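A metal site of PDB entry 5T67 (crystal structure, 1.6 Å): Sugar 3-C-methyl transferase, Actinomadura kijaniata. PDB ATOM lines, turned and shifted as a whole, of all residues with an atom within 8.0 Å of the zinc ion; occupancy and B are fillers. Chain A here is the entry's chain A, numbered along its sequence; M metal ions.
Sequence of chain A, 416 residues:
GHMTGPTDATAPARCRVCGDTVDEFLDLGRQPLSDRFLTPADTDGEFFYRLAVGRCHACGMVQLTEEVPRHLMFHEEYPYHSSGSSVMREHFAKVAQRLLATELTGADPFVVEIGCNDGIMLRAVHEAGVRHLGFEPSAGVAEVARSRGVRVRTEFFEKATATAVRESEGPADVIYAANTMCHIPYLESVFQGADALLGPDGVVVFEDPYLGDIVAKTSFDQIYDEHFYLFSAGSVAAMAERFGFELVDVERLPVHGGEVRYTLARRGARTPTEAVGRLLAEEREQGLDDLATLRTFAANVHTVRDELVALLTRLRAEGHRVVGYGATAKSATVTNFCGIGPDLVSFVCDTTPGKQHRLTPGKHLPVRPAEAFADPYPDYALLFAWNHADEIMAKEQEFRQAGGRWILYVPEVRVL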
ATOM      1  N   ARG A  14     -14.870  -0.585 -16.686  1.00  0.00           N
ATOM      2  CA  ARG A  14     -15.058  -1.647 -17.684  1.00  0.00           C
ATOM      3  C   ARG A  14     -16.382  -2.372 -17.508  1.00  0.00           C
ATOM      4  O   ARG A  14     -16.840  -2.643 -16.388  1.00  0.00           O
ATOM      5  CB  ARG A  14     -13.873  -2.608 -17.705  1.00  0.00           C
ATOM      6  CG  ARG A  14     -12.558  -1.860 -17.919  1.00  0.00           C
ATOM      7  CD  ARG A  14     -11.587  -2.621 -18.797  1.00  0.00           C
ATOM      8  NE  ARG A  14     -11.926  -2.386 -20.198  1.00  0.00           N
ATOM      9  CZ  ARG A  14     -11.057  -2.334 -21.209  1.00  0.00           C
ATOM     10  NH1 ARG A  14     -11.483  -2.117 -22.445  1.00  0.00           N
ATOM     11  NH2 ARG A  14      -9.751  -2.497 -21.013  1.00  0.00           N
ATOM     12  N   CYS A  15     -16.991  -2.670 -18.638  1.00  0.00           N
ATOM     13  CA  CYS A  15     -18.279  -3.319 -18.625  1.00  0.00           C
ATOM     14  C   CYS A  15     -18.241  -4.684 -17.940  1.00  0.00           C
ATOM     15  O   CYS A  15     -17.395  -5.517 -18.257  1.00  0.00           O
ATOM     16  CB  CYS A  15     -18.716  -3.505 -20.068  1.00  0.00           C
ATOM     17  SG  CYS A  15     -20.291  -4.357 -20.237  1.00  0.00           S
ATOM     18  N   ARG A  16     -19.178  -4.978 -17.055  1.00  0.00           N
ATOM     19  CA  ARG A  16     -19.260  -6.283 -16.391  1.00  0.00           C
ATOM     20  C   ARG A  16     -19.773  -7.415 -17.269  1.00  0.00           C
ATOM     21  O   ARG A  16     -19.716  -8.574 -16.857  1.00  0.00           O
ATOM     22  CB  ARG A  16     -20.143  -6.247 -15.132  1.00  0.00           C
ATOM     23  CG  ARG A  16     -19.462  -5.952 -13.818  1.00  0.00           C
ATOM     24  CD  ARG A  16     -18.327  -6.878 -13.446  1.00  0.00           C
ATOM     25  NE  ARG A  16     -18.633  -8.027 -12.578  1.00  0.00           N
ATOM     26  CZ  ARG A  16     -18.703  -9.285 -13.025  1.00  0.00           C
ATOM     27  NH1 ARG A  16     -18.921 -10.279 -12.179  1.00  0.00           N
ATOM     28  NH2 ARG A  16     -18.533  -9.568 -14.329  1.00  0.00           N
ATOM     29  N   VAL A  17     -20.314  -7.095 -18.452  1.00  0.00           N
ATOM     30  CA  VAL A  17     -20.788  -8.102 -19.367  1.00  0.00           C
ATOM     31  C   VAL A  17     -19.663  -8.398 -20.337  1.00  0.00           C
ATOM     32  O   VAL A  17     -19.261  -9.575 -20.423  1.00  0.00           O
ATOM     33  CB  VAL A  17     -22.086  -7.706 -20.045  1.00  0.00           C
ATOM     34  CG1 VAL A  17     -22.522  -8.675 -21.146  1.00  0.00           C
ATOM     35  CG2 VAL A  17     -23.152  -7.557 -18.985  1.00  0.00           C
ATOM     36  N   CYS A  18     -19.112  -7.390 -21.015  1.00  0.00           N
ATOM     37  CA  CYS A  18     -18.172  -7.711 -22.096  1.00  0.00           C
ATOM     38  C   CYS A  18     -16.730  -7.279 -21.881  1.00  0.00           C
ATOM     39  O   CYS A  18     -15.822  -7.637 -22.675  1.00  0.00           O
ATOM     40  CB  CYS A  18     -18.693  -7.150 -23.387  1.00  0.00           C
ATOM     41  SG  CYS A  18     -18.498  -5.411 -23.685  1.00  0.00           S
ATOM     42  N   GLY A  19     -16.488  -6.502 -20.825  1.00  0.00           N
ATOM     43  CA  GLY A  19     -15.155  -6.015 -20.469  1.00  0.00           C
ATOM     44  C   GLY A  19     -14.655  -4.800 -21.223  1.00  0.00           C
ATOM     45  O   GLY A  19     -13.490  -4.422 -21.055  1.00  0.00           O
ATOM     46  N   ASP A  20     -15.478  -4.204 -22.092  1.00  0.00           N
ATOM     47  CA  ASP A  20     -15.032  -2.985 -22.797  1.00  0.00           C
ATOM     48  C   ASP A  20     -15.350  -1.741 -21.967  1.00  0.00           C
ATOM     49  O   ASP A  20     -15.774  -1.834 -20.809  1.00  0.00           O
ATOM     50  CB  ASP A  20     -15.677  -2.921 -24.188  1.00  0.00           C
ATOM     51  CG  ASP A  20     -14.759  -2.321 -25.248  1.00  0.00           C
ATOM     52  OD1 ASP A  20     -14.752  -2.844 -26.379  1.00  0.00           O
ATOM     53  OD2 ASP A  20     -14.054  -1.343 -24.957  1.00  0.00           O
ATOM     54  N   THR A  21     -15.119  -0.570 -22.536  1.00  0.00           N
ATOM     55  CA  THR A  21     -15.114   0.658 -21.773  1.00  0.00           C
ATOM     56  C   THR A  21     -16.517   1.261 -21.633  1.00  0.00           C
ATOM     57  O   THR A  21     -17.294   1.353 -22.585  1.00  0.00           O
ATOM     58  CB  THR A  21     -14.110   1.698 -22.327  1.00  0.00           C
ATOM     59  OG1 THR A  21     -14.308   1.916 -23.724  1.00  0.00           O
ATOM     60  CG2 THR A  21     -12.683   1.171 -22.178  1.00  0.00           C
ATOM     61  N   VAL A  22     -16.786   1.728 -20.408  1.00  0.00           N
ATOM     62  CA  VAL A  22     -18.109   2.273 -20.038  1.00  0.00           C
ATOM     63  C   VAL A  22     -17.935   3.780 -19.997  1.00  0.00           C
ATOM     64  O   VAL A  22     -16.985   4.263 -19.367  1.00  0.00           O
ATOM     65  CB  VAL A  22     -18.573   1.738 -18.670  1.00  0.00           C
ATOM     66  CG1 VAL A  22     -19.777   2.524 -18.153  1.00  0.00           C
ATOM     67  CG2 VAL A  22     -18.904   0.264 -18.797  1.00  0.00           C
ATOM     68  N   ARG A  55     -22.734   3.725 -19.710  1.00  0.00           N
ATOM     69  CA  ARG A  55     -23.183   2.917 -20.818  1.00  0.00           C
ATOM     70  C   ARG A  55     -21.956   2.273 -21.462  1.00  0.00           C
ATOM     71  O   ARG A  55     -21.012   2.964 -21.829  1.00  0.00           O
ATOM     72  CB  ARG A  55     -23.966   3.745 -21.805  1.00  0.00           C
ATOM     73  CG  ARG A  55     -24.440   2.882 -22.979  1.00  0.00           C
ATOM     74  CD  ARG A  55     -25.109   3.710 -24.042  1.00  0.00           C
ATOM     75  NE  ARG A  55     -25.990   2.898 -24.899  1.00  0.00           N
ATOM     76  CZ  ARG A  55     -25.573   2.273 -26.000  1.00  0.00           C
ATOM     77  NH1 ARG A  55     -24.296   2.410 -26.372  1.00  0.00           N
ATOM     78  NH2 ARG A  55     -26.392   1.521 -26.728  1.00  0.00           N
ATOM     79  N   CYS A  56     -21.930   0.938 -21.570  1.00  0.00           N
ATOM     80  CA  CYS A  56     -20.828   0.290 -22.310  1.00  0.00           C
ATOM     81  C   CYS A  56     -20.849   0.736 -23.739  1.00  0.00           C
ATOM     82  O   CYS A  56     -21.878   0.634 -24.378  1.00  0.00           O
ATOM     83  CB  CYS A  56     -20.974  -1.231 -22.302  1.00  0.00           C
ATOM     84  SG  CYS A  56     -19.629  -2.069 -23.219  1.00  0.00           S
ATOM     85  N   HIS A  57     -19.752   1.206 -24.299  1.00  0.00           N
ATOM     86  CA  HIS A  57     -19.827   1.718 -25.684  1.00  0.00           C
ATOM     87  C   HIS A  57     -19.932   0.580 -26.715  1.00  0.00           C
ATOM     88  O   HIS A  57     -20.394   0.805 -27.822  1.00  0.00           O
ATOM     89  CB  HIS A  57     -18.661   2.641 -26.001  1.00  0.00           C
ATOM     90  CG  HIS A  57     -17.441   1.932 -26.470  1.00  0.00           C
ATOM     91  ND1 HIS A  57     -16.499   1.400 -25.610  1.00  0.00           N
ATOM     92  CD2 HIS A  57     -17.004   1.652 -27.721  1.00  0.00           C
ATOM     93  CE1 HIS A  57     -15.541   0.834 -26.309  1.00  0.00           C
ATOM     94  NE2 HIS A  57     -15.822   0.959 -27.588  1.00  0.00           N
ATOM     95  N   ALA A  58     -19.552  -0.628 -26.333  1.00  0.00           N
ATOM     96  CA  ALA A  58     -19.563  -1.796 -27.221  1.00  0.00           C
ATOM     97  C   ALA A  58     -20.854  -2.547 -27.298  1.00  0.00           C
ATOM     98  O   ALA A  58     -21.450  -2.670 -28.371  1.00  0.00           O
ATOM     99  CB  ALA A  58     -18.438  -2.742 -26.842  1.00  0.00           C
ATOM    100  N   CYS A  59     -21.310  -3.003 -26.133  1.00  0.00           N
ATOM    101  CA  CYS A  59     -22.498  -3.798 -26.027  1.00  0.00           C
ATOM    102  C   CYS A  59     -23.729  -3.015 -25.592  1.00  0.00           C
ATOM    103  O   CYS A  59     -24.856  -3.502 -25.658  1.00  0.00           O
ATOM    104  CB  CYS A  59     -22.237  -4.979 -25.075  1.00  0.00           C
ATOM    105  SG  CYS A  59     -22.391  -4.533 -23.334  1.00  0.00           S
ATOM    106  N   GLY A  60     -23.509  -1.796 -25.122  1.00  0.00           N
ATOM    107  CA  GLY A  60     -24.655  -0.950 -24.818  1.00  0.00           C
ATOM    108  C   GLY A  60     -25.240  -1.079 -23.409  1.00  0.00           C
ATOM    109  O   GLY A  60     -26.157  -0.303 -23.041  1.00  0.00           O
ATOM    110  N   MET A  61     -24.784  -2.058 -22.641  1.00  0.00           N
ATOM    111  CA  MET A  61     -25.343  -2.310 -21.313  1.00  0.00           C
ATOM    112  C   MET A  61     -25.114  -1.078 -20.408  1.00  0.00           C
ATOM    113  O   MET A  61     -23.995  -0.607 -20.164  1.00  0.00           O
ATOM    114  CB  MET A  61     -24.735  -3.546 -20.661  1.00  0.00           C
ATOM    115  CG  MET A  61     -25.313  -3.892 -19.301  1.00  0.00           C
ATOM    116  SD  MET A  61     -27.059  -4.338 -19.452  1.00  0.00           S
ATOM    117  CE  MET A  61     -27.027  -5.983 -20.150  1.00  0.00           C
ATOM    118  N   VAL A  62     -26.204  -0.594 -19.853  1.00  0.00           N
ATOM    119  CA  VAL A  62     -26.195   0.528 -18.908  1.00  0.00           C
ATOM    120  C   VAL A  62     -26.057  -0.102 -17.521  1.00  0.00           C
ATOM    121  O   VAL A  62     -26.753  -1.067 -17.156  1.00  0.00           O
ATOM    122  CB  VAL A  62     -27.502   1.373 -18.984  1.00  0.00           C
ATOM    123  CG1 VAL A  62     -27.651   2.360 -17.807  1.00  0.00           C
ATOM    124  CG2 VAL A  62     -27.444   2.094 -20.314  1.00  0.00           C
ATOM    125  N   GLN A  63     -25.156   0.434 -16.718  1.00  0.00           N
ATOM    126  CA  GLN A  63     -24.738  -0.262 -15.514  1.00  0.00           C
ATOM    127  C   GLN A  63     -24.065   0.706 -14.553  1.00  0.00           C
ATOM    128  O   GLN A  63     -23.570   1.777 -14.937  1.00  0.00           O
ATOM    129  CB  GLN A  63     -23.739  -1.389 -15.760  1.00  0.00           C
ATOM    130  CG  GLN A  63     -22.521  -0.917 -16.526  1.00  0.00           C
ATOM    131  CD  GLN A  63     -21.739  -2.027 -17.252  1.00  0.00           C
ATOM    132  OE1 GLN A  63     -20.943  -2.713 -16.623  1.00  0.00           O
ATOM    133  NE2 GLN A  63     -22.014  -2.244 -18.530  1.00  0.00           N
ATOM    134  N   ALA A 238     -27.946  -8.348 -26.774  1.00  0.00           N
ATOM    135  CA  ALA A 238     -26.493  -8.475 -26.940  1.00  0.00           C
ATOM    136  C   ALA A 238     -25.924  -9.377 -25.868  1.00  0.00           C
ATOM    137  O   ALA A 238     -25.088 -10.274 -26.151  1.00  0.00           O
ATOM    138  CB  ALA A 238     -25.825  -7.114 -26.908  1.00  0.00           C
ATOM    139  N   ARG A 242     -23.960 -13.061 -26.427  1.00  0.00           N
ATOM    140  CA  ARG A 242     -22.673 -13.282 -25.795  1.00  0.00           C
ATOM    141  C   ARG A 242     -22.593 -14.588 -24.973  1.00  0.00           C
ATOM    142  O   ARG A 242     -21.593 -15.310 -25.011  1.00  0.00           O
ATOM    143  CB  ARG A 242     -22.262 -12.103 -24.917  1.00  0.00           C
ATOM    144  CG  ARG A 242     -21.001 -12.420 -24.123  1.00  0.00           C
ATOM    145  CD  ARG A 242     -20.391 -11.239 -23.427  1.00  0.00           C
ATOM    146  NE  ARG A 242     -20.458 -10.162 -24.400  1.00  0.00           N
ATOM    147  CZ  ARG A 242     -19.451  -9.728 -25.139  1.00  0.00           C
ATOM    148  NH1 ARG A 242     -19.682  -8.754 -26.007  1.00  0.00           N
ATOM    149  NH2 ARG A 242     -18.226 -10.232 -24.966  1.00  0.00           N
HETATM  150 ZN    ZN M   1     -20.266  -4.220 -22.696  1.00  0.00          ZN
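The backbone carbonyl oxygen of Asp 20 is in hydrogen-bond range of the backbone NH of Cys 15 (2.6 Å).
The side-chain sulfur (SG) of Cys 59 sits close to the backbone NH (N) of Met 61 (3.5 Å).
The backbone NH (N) of Cys 56 is in hydrogen-bond range of the backbone carbonyl oxygen (O) of Met 61 (2.9 Å).
The side-chain sulfur (SG) of Cys 18 sits close to the backbone NH (N) of Asp 20, at 3.6 Å.
The side-chain sulfur (SG) of Cys 15 lies close to the backbone NH (N) of Val 17 (3.3 Å).
The side-chain sulfur (SG) of Cys 15 lies close to the side-chain amide nitrogen (NE2) of Gln 63 (3.2 Å).
The side-chain sulfur of Cys 56 sits close to the backbone NH of Ala 58 (3.4 Å).
The nearest printed residue that does not touch the zinc ion is Gly 60 (4.7 Å).
SG of Cys 59 binds the zinc ion (2.2 Å).
The side-chain sulfur (SG) of Cys 56 binds the zinc ion.
The zinc ion is bound by SG of Cys 18 (2.3 Å).
SG of Cys 15 is bound to the zinc ion (2.5 Å).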
